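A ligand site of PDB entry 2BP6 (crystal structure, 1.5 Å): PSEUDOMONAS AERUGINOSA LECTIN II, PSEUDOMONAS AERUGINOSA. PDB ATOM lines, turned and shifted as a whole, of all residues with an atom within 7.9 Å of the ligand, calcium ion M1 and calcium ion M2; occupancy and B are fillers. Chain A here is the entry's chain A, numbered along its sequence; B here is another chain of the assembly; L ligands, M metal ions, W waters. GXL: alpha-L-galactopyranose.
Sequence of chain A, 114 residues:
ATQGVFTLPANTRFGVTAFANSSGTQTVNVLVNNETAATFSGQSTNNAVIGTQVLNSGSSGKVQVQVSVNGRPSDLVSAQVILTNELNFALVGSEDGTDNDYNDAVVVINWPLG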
ATOM      1  N   ALA A  20     -20.329  25.517  17.985  1.00  0.00           N
ATOM      2  CA  ALA A  20     -21.324  24.482  18.297  1.00  0.00           C
ATOM      3  C   ALA A  20     -22.056  24.022  17.057  1.00  0.00           C
ATOM      4  O   ALA A  20     -22.393  24.831  16.168  1.00  0.00           O
ATOM      5  CB  ALA A  20     -22.327  25.019  19.324  1.00  0.00           C
ATOM      6  N   ASN A  21     -22.292  22.704  17.002  1.00  0.00           N
ATOM      7  CA  ASN A  21     -23.058  22.085  15.904  1.00  0.00           C
ATOM      8  C   ASN A  21     -23.879  20.916  16.451  1.00  0.00           C
ATOM      9  O   ASN A  21     -23.562  19.738  16.191  1.00  0.00           O
ATOM     10  CB  ASN A  21     -22.135  21.547  14.803  1.00  0.00           C
ATOM     11  CG  ASN A  21     -21.456  22.658  14.040  1.00  0.00           C
ATOM     12  OD1 ASN A  21     -22.044  23.285  13.169  1.00  0.00           O
ATOM     13  ND2 ASN A  21     -20.202  22.910  14.389  1.00  0.00           N
ATOM     14  N   SER A  22     -24.928  21.222  17.206  1.00  0.00           N
ATOM     15  CA  SER A  22     -25.697  20.154  17.847  1.00  0.00           C
ATOM     16  C   SER A  22     -26.986  20.715  18.391  1.00  0.00           C
ATOM     17  O   SER A  22     -27.069  21.914  18.676  1.00  0.00           O
ATOM     18  CB  SER A  22     -24.891  19.603  19.031  1.00  0.00           C
ATOM     19  OG  SER A  22     -25.676  18.685  19.809  1.00  0.00           O
ATOM     20  N   SER A  23     -27.982  19.855  18.565  1.00  0.00           N
ATOM     21  CA  SER A  23     -29.208  20.243  19.276  1.00  0.00           C
ATOM     22  C   SER A  23     -28.969  20.552  20.746  1.00  0.00           C
ATOM     23  O   SER A  23     -29.776  21.255  21.371  1.00  0.00           O
ATOM     24  CB  SER A  23     -30.263  19.155  19.143  1.00  0.00           C
ATOM     25  OG  SER A  23     -30.901  19.248  17.895  1.00  0.00           O
ATOM     26  N   GLY A  24     -27.891  20.005  21.280  1.00  0.00           N
ATOM     27  CA  GLY A  24     -27.591  20.176  22.702  1.00  0.00           C
ATOM     28  C   GLY A  24     -26.728  21.369  23.062  1.00  0.00           C
ATOM     29  O   GLY A  24     -25.849  21.775  22.308  1.00  0.00           O
ATOM     30  N   GLN A  26     -23.732  23.089  24.507  1.00  0.00           N
ATOM     31  CA  GLN A  26     -22.354  22.662  24.796  1.00  0.00           C
ATOM     32  C   GLN A  26     -21.746  23.502  25.910  1.00  0.00           C
ATOM     33  O   GLN A  26     -21.903  24.719  25.904  1.00  0.00           O
ATOM     34  CB  GLN A  26     -21.480  22.873  23.535  1.00  0.00           C
ATOM     35  CG  GLN A  26     -22.110  22.312  22.274  1.00  0.00           C
ATOM     36  CD  GLN A  26     -22.127  20.785  22.285  1.00  0.00           C
ATOM     37  OE1 GLN A  26     -21.078  20.145  22.450  1.00  0.00           O
ATOM     38  NE2 GLN A  26     -23.322  20.184  22.061  1.00  0.00           N
ATOM     39  N   GLN A  43     -25.598  27.073  22.282  1.00  0.00           N
ATOM     40  CA  GLN A  43     -26.252  26.076  21.476  1.00  0.00           C
ATOM     41  C   GLN A  43     -26.395  26.610  20.068  1.00  0.00           C
ATOM     42  O   GLN A  43     -26.890  27.735  19.873  1.00  0.00           O
ATOM     43  CB  GLN A  43     -27.636  25.772  22.058  1.00  0.00           C
ATOM     44  CG  GLN A  43     -28.308  24.577  21.350  1.00  0.00           C
ATOM     45  CD  GLN A  43     -29.037  24.988  20.079  1.00  0.00           C
ATOM     46  OE1 GLN A  43     -29.677  26.039  20.031  1.00  0.00           O
ATOM     47  NE2 GLN A  43     -28.929  24.171  19.026  1.00  0.00           N
ATOM     48  N   SER A  44     -25.983  25.807  19.089  1.00  0.00           N
ATOM     49  CA  SER A  44     -26.155  26.163  17.676  1.00  0.00           C
ATOM     50  C   SER A  44     -26.089  24.891  16.829  1.00  0.00           C
ATOM     51  O   SER A  44     -25.322  23.980  17.165  1.00  0.00           O
ATOM     52  CB  SER A  44     -25.000  27.096  17.253  1.00  0.00           C
ATOM     53  OG  SER A  44     -25.102  27.434  15.876  1.00  0.00           O
ATOM     54  N   THR A  45     -26.829  24.854  15.731  1.00  0.00           N
ATOM     55  CA  THR A  45     -26.621  23.817  14.720  1.00  0.00           C
ATOM     56  C   THR A  45     -26.014  24.405  13.462  1.00  0.00           C
ATOM     57  O   THR A  45     -26.014  23.780  12.433  1.00  0.00           O
ATOM     58  CB  THR A  45     -27.927  23.071  14.336  1.00  0.00           C
ATOM     59  OG1 THR A  45     -28.978  24.024  14.109  1.00  0.00           O
ATOM     60  CG2 THR A  45     -28.337  22.090  15.446  1.00  0.00           C
ATOM     61  N   VAL A  69     -22.120  17.916  27.680  1.00  0.00           N
ATOM     62  CA  VAL A  69     -23.451  18.165  27.079  1.00  0.00           C
ATOM     63  C   VAL A  69     -24.460  17.291  27.804  1.00  0.00           C
ATOM     64  O   VAL A  69     -24.220  16.108  28.026  1.00  0.00           O
ATOM     65  CB  VAL A  69     -23.486  17.826  25.565  1.00  0.00           C
ATOM     66  CG1 VAL A  69     -24.871  18.206  24.940  1.00  0.00           C
ATOM     67  CG2 VAL A  69     -22.361  18.537  24.813  1.00  0.00           C
ATOM     68  N   SER A  94     -15.663  16.879  19.195  1.00  0.00           N
ATOM     69  CA  SER A  94     -16.351  16.200  20.290  1.00  0.00           C
ATOM     70  C   SER A  94     -17.691  15.654  19.816  1.00  0.00           C
ATOM     71  O   SER A  94     -18.301  16.235  18.909  1.00  0.00           O
ATOM     72  CB  SER A  94     -16.537  17.131  21.509  1.00  0.00           C
ATOM     73  OG  SER A  94     -17.372  18.245  21.199  1.00  0.00           O
ATOM     74  N   GLU A  95     -18.118  14.531  20.403  1.00  0.00           N
ATOM     75  CA  GLU A  95     -19.355  13.837  20.047  1.00  0.00           C
ATOM     76  C   GLU A  95     -20.201  13.689  21.294  1.00  0.00           C
ATOM     77  O   GLU A  95     -19.782  13.042  22.264  1.00  0.00           O
ATOM     78  CB  GLU A  95     -19.034  12.467  19.483  1.00  0.00           C
ATOM     79  CG  GLU A  95     -20.281  11.675  19.076  1.00  0.00           C
ATOM     80  CD  GLU A  95     -21.209  12.487  18.175  1.00  0.00           C
ATOM     81  OE1 GLU A  95     -20.750  13.067  17.169  1.00  0.00           O
ATOM     82  OE2 GLU A  95     -22.416  12.601  18.477  1.00  0.00           O
ATOM     83  N   ASP A  96     -21.416  14.277  21.233  1.00  0.00           N
ATOM     84  CA  ASP A  96     -22.345  14.244  22.362  1.00  0.00           C
ATOM     85  C   ASP A  96     -23.454  13.216  22.215  1.00  0.00           C
ATOM     86  O   ASP A  96     -24.305  13.092  23.109  1.00  0.00           O
ATOM     87  CB  ASP A  96     -22.951  15.647  22.592  1.00  0.00           C
ATOM     88  CG  ASP A  96     -23.851  16.142  21.457  1.00  0.00           C
ATOM     89  OD1 ASP A  96     -24.434  15.313  20.719  1.00  0.00           O
ATOM     90  OD2 ASP A  96     -24.049  17.382  21.392  1.00  0.00           O
ATOM     91  N   GLY A  97     -23.417  12.475  21.103  1.00  0.00           N
ATOM     92  CA  GLY A  97     -24.545  11.636  20.710  1.00  0.00           C
ATOM     93  C   GLY A  97     -24.099  10.364  20.049  1.00  0.00           C
ATOM     94  O   GLY A  97     -23.112   9.743  20.453  1.00  0.00           O
ATOM     95  N   THR A  98     -24.834   9.994  19.002  1.00  0.00           N
ATOM     96  CA  THR A  98     -24.637   8.691  18.374  1.00  0.00           C
ATOM     97  C   THR A  98     -24.221   8.754  16.912  1.00  0.00           C
ATOM     98  O   THR A  98     -23.821   7.720  16.363  1.00  0.00           O
ATOM     99  CB  THR A  98     -25.899   7.815  18.505  1.00  0.00           C
ATOM    100  OG1 THR A  98     -26.992   8.447  17.844  1.00  0.00           O
ATOM    101  CG2 THR A  98     -26.291   7.593  19.988  1.00  0.00           C
ATOM    102  N   ASP A  99     -24.323   9.940  16.276  1.00  0.00           N
ATOM    103  CA  ASP A  99     -24.098  10.029  14.830  1.00  0.00           C
ATOM    104  C   ASP A  99     -22.622  10.095  14.474  1.00  0.00           C
ATOM    105  O   ASP A  99     -22.261   9.914  13.313  1.00  0.00           O
ATOM    106  CB  ASP A  99     -24.897  11.180  14.169  1.00  0.00           C
ATOM    107  CG  ASP A  99     -24.393  12.581  14.583  1.00  0.00           C
ATOM    108  OD1 ASP A  99     -23.608  12.657  15.563  1.00  0.00           O
ATOM    109  OD2 ASP A  99     -24.867  13.539  13.902  1.00  0.00           O
ATOM    110  N   ASN A 100     -21.790  10.372  15.469  1.00  0.00           N
ATOM    111  CA  ASN A 100     -20.337  10.354  15.270  1.00  0.00           C
ATOM    112  C   ASN A 100     -19.864  11.347  14.233  1.00  0.00           C
ATOM    113  O   ASN A 100     -18.921  11.060  13.473  1.00  0.00           O
ATOM    114  CB  ASN A 100     -19.868   8.928  14.989  1.00  0.00           C
ATOM    115  CG  ASN A 100     -20.029   8.057  16.205  1.00  0.00           C
ATOM    116  OD1 ASN A 100     -20.080   8.559  17.335  1.00  0.00           O
ATOM    117  ND2 ASN A 100     -20.139   6.745  15.996  1.00  0.00           N
ATOM    118  N   ASP A 101     -20.500  12.505  14.172  1.00  0.00           N
ATOM    119  CA  ASP A 101     -19.961  13.604  13.349  1.00  0.00           C
ATOM    120  C   ASP A 101     -18.807  14.362  14.029  1.00  0.00           C
ATOM    121  O   ASP A 101     -18.017  15.016  13.324  1.00  0.00           O
ATOM    122  CB  ASP A 101     -21.039  14.545  12.754  1.00  0.00           C
ATOM    123  CG  ASP A 101     -21.857  15.318  13.797  1.00  0.00           C
ATOM    124  OD1 ASP A 101     -21.657  15.109  15.033  1.00  0.00           O
ATOM    125  OD2 ASP A 101     -22.678  16.153  13.328  1.00  0.00           O
ATOM    126  N   TYR A 102     -18.726  14.255  15.365  1.00  0.00           N
ATOM    127  CA  TYR A 102     -17.594  14.815  16.122  1.00  0.00           C
ATOM    128  C   TYR A 102     -17.449  16.325  15.985  1.00  0.00           C
ATOM    129  O   TYR A 102     -16.381  16.875  16.272  1.00  0.00           O
ATOM    130  CB  TYR A 102     -16.260  14.056  15.830  1.00  0.00           C
ATOM    131  CG  TYR A 102     -16.216  12.787  16.687  1.00  0.00           C
ATOM    132  CD1 TYR A 102     -16.820  11.595  16.250  1.00  0.00           C
ATOM    133  CD2 TYR A 102     -15.708  12.837  17.998  1.00  0.00           C
ATOM    134  CE1 TYR A 102     -16.841  10.474  17.084  1.00  0.00           C
ATOM    135  CE2 TYR A 102     -15.729  11.704  18.819  1.00  0.00           C
ATOM    136  CZ  TYR A 102     -16.308  10.550  18.353  1.00  0.00           C
ATOM    137  OH  TYR A 102     -16.370   9.429  19.165  1.00  0.00           O
ATOM    138  N   ASN A 103     -18.543  16.999  15.625  1.00  0.00           N
ATOM    139  CA  ASN A 103     -18.474  18.465  15.471  1.00  0.00           C
ATOM    140  C   ASN A 103     -19.345  19.195  16.492  1.00  0.00           C
ATOM    141  O   ASN A 103     -19.597  20.382  16.362  1.00  0.00           O
ATOM    142  CB  ASN A 103     -18.897  18.848  14.036  1.00  0.00           C
ATOM    143  CG  ASN A 103     -20.389  18.663  13.802  1.00  0.00           C
ATOM    144  OD1 ASN A 103     -21.103  18.225  14.721  1.00  0.00           O
ATOM    145  ND2 ASN A 103     -20.878  19.016  12.596  1.00  0.00           N
ATOM    146  N   ASP A 104     -19.826  18.464  17.499  1.00  0.00           N
ATOM    147  CA  ASP A 104     -20.891  19.015  18.311  1.00  0.00           C
ATOM    148  C   ASP A 104     -20.414  20.233  19.086  1.00  0.00           C
ATOM    149  O   ASP A 104     -21.114  21.236  19.213  1.00  0.00           O
ATOM    150  CB  ASP A 104     -21.446  17.894  19.211  1.00  0.00           C
ATOM    151  CG  ASP A 104     -22.028  16.753  18.400  1.00  0.00           C
ATOM    152  OD1 ASP A 104     -22.604  17.008  17.322  1.00  0.00           O
ATOM    153  OD2 ASP A 104     -21.883  15.583  18.830  1.00  0.00           O
ATOM    154  N   ALA A 105     -19.206  20.122  19.603  1.00  0.00           N
ATOM    155  CA  ALA A 105     -18.396  21.309  19.917  1.00  0.00           C
ATOM    156  C   ALA A 105     -17.048  21.107  19.239  1.00  0.00           C
ATOM    157  O   ALA A 105     -16.451  20.030  19.345  1.00  0.00           O
ATOM    158  CB  ALA A 105     -18.193  21.491  21.419  1.00  0.00           C
ATOM    159  N   PRO B 112     -17.741  18.621   8.675  1.00  0.00           N
ATOM    160  CA  PRO B 112     -19.096  19.060   8.436  1.00  0.00           C
ATOM    161  C   PRO B 112     -19.626  19.919   9.581  1.00  0.00           C
ATOM    162  O   PRO B 112     -19.085  19.956  10.689  1.00  0.00           O
ATOM    163  CB  PRO B 112     -19.891  17.741   8.387  1.00  0.00           C
ATOM    164  CG  PRO B 112     -19.144  16.846   9.351  1.00  0.00           C
ATOM    165  CD  PRO B 112     -17.660  17.227   9.133  1.00  0.00           C
ATOM    166  N   LEU B 113     -20.716  20.618   9.268  1.00  0.00           N
ATOM    167  CA  LEU B 113     -21.483  21.388  10.241  1.00  0.00           C
ATOM    168  C   LEU B 113     -22.784  20.659  10.575  1.00  0.00           C
ATOM    169  O   LEU B 113     -23.121  19.613   9.972  1.00  0.00           O
ATOM    170  CB  LEU B 113     -21.847  22.756   9.670  1.00  0.00           C
ATOM    171  CG  LEU B 113     -20.664  23.568   9.129  1.00  0.00           C
ATOM    172  CD1 LEU B 113     -21.148  24.967   8.835  1.00  0.00           C
ATOM    173  CD2 LEU B 113     -19.532  23.614  10.166  1.00  0.00           C
ATOM    174  N   GLY B 114     -23.537  21.241  11.508  1.00  0.00           N
ATOM    175  CA  GLY B 114     -24.875  20.757  11.853  1.00  0.00           C
ATOM    176  C   GLY B 114     -24.956  19.657  12.884  1.00  0.00           C
ATOM    177  O   GLY B 114     -23.930  19.024  13.201  1.00  0.00           O
ATOM    178  OXT GLY B 114     -26.058  19.368  13.367  1.00  0.00           O
HETATM  179  C1  GXL L   1     -27.079  16.161  18.165  1.00  0.00           C
HETATM  180  C2  GXL L   1     -25.687  15.949  17.550  1.00  0.00           C
HETATM  181  C3  GXL L   1     -25.831  15.603  16.078  1.00  0.00           C
HETATM  182  C4  GXL L   1     -26.628  16.686  15.385  1.00  0.00           C
HETATM  183  C5  GXL L   1     -27.968  16.881  16.084  1.00  0.00           C
HETATM  184  C6  GXL L   1     -28.746  18.054  15.495  1.00  0.00           C
HETATM  185  O1  GXL L   1     -27.807  14.927  18.065  1.00  0.00           O
HETATM  186  O2  GXL L   1     -24.952  14.888  18.178  1.00  0.00           O
HETATM  187  O3  GXL L   1     -24.508  15.490  15.493  1.00  0.00           O
HETATM  188  O4  GXL L   1     -25.810  17.881  15.366  1.00  0.00           O
HETATM  189  O5  GXL L   1     -27.754  17.187  17.463  1.00  0.00           O
HETATM  190  O6  GXL L   1     -29.182  17.711  14.186  1.00  0.00           O
HETATM  191 CA    CA M   1     -22.824  14.395  16.959  1.00  0.00          CA
HETATM  192 CA    CA M   2     -23.321  17.633  15.156  1.00  0.00          CA
HETATM  193  O   HOH W   1     -29.826  15.190  13.409  1.00  0.00           O
HETATM  194  O   HOH W   2     -28.453  19.950  12.368  1.00  0.00           O
HETATM  195  O   HOH W   3     -26.313  12.226  17.562  1.00  0.00           O
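ND2 of Asn 103 sits at hydrogen-bond distance from O of Pro 112 of chain B, 2.8 Å away. The backbone NH (N) of Asp 96 sits close to the side-chain carboxylate (OD2) of Asp 104. The backbone NH (N) of Asp 104 is in hydrogen-bond range of the backbone carbonyl oxygen (O) of Ser 94. OE1 of Gln 26 sits close to O of Asp 104 (3.4 Å). The backbone NH (N) of Gly 97 sits close to the side-chain carboxylate (OE2) of Glu 95 (2.8 Å). The side-chain amide nitrogen (NE2) of Gln 26 lies within hydrogen-bond range of the side-chain carboxylate (OD2) of Asp 96, at 3.0 Å. OG of Ser 22 lies within hydrogen-bond range of N of Gly 24, 3.0 Å away. The backbone NH (N) of Ser 22 is in hydrogen-bond range of the backbone carbonyl oxygen (O) of Ser 44 (2.8 Å).
Nine residues have an atom within 4 Å of the ligand: Asn 21, Ser 22, Ser 23, Glu 95, Asp 96, Asp 99, Asp 101, Asp 104 and Gly 114 of chain B. Along chain A the residues within 4 Å of the ligand span positions 21 to 104.
Of the 25 residues printed, 4 come within 4 Å of calcium ion M1.
OD1 of Asp 101 is bound to calcium ion M1 (2.4 Å). Calcium ion M1 is bound by OD1 of Asp 99 (2.4 Å). OE2 of Glu 95 binds calcium ion M1 (2.4 Å). Calcium ion M1 is bound by OD2 of Asp 104, 2.4 Å away. OE1 of Glu 95 is bound to calcium ion M1, 2.5 Å away. Calcium ion M1 is bound by O3 of the ligand (2.5 Å). O2 of the ligand is bound to calcium ion M1. Calcium ion M1 is bound by OD1 of Asp 104, 2.6 Å away.
The nearest printed residue that does not touch calcium ion M2 is Ser 22 (4.4 Å).
Calcium ion M2 is bound by the side-chain amide oxygen (OD1) of Asn 103 (2.3 Å), the backbone carbonyl oxygen (O) of Asn 21 (2.4 Å), the side-chain carboxylate (OD1) of Asp 104 (2.4 Å), the side-chain carboxylate (OD2) of Asp 101 (2.4 Å), an oxygen (O3) of the ligand (2.5 Å), the chain-end carboxylate (O) of Gly 114 of chain B (2.5 Å) and an oxygen (O4) of the ligand (2.5 Å). Slightly farther from calcium ion M2 lies the side-chain carboxylate (OD1) of Asp 101 (3.0 Å).
O2 of the ligand lies close to OD1 of Asp 96, 2.6 Å away. N of Ser 23 lies within hydrogen-bond range of O5 of the ligand (2.9 Å). The side-chain hydroxyl (OG) of Ser 22 lies close to an oxygen (O5) of the ligand (3.5 Å).
Water W2 bridges OXT of Gly 114 of chain B (2.7 Å) and O6 of the ligand (3.0 Å). Water W3 lies within hydrogen-bond range of the backbone NH (N) of Thr 98, an oxygen (O1) of the ligand and the backbone NH (N) of Asp 99.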
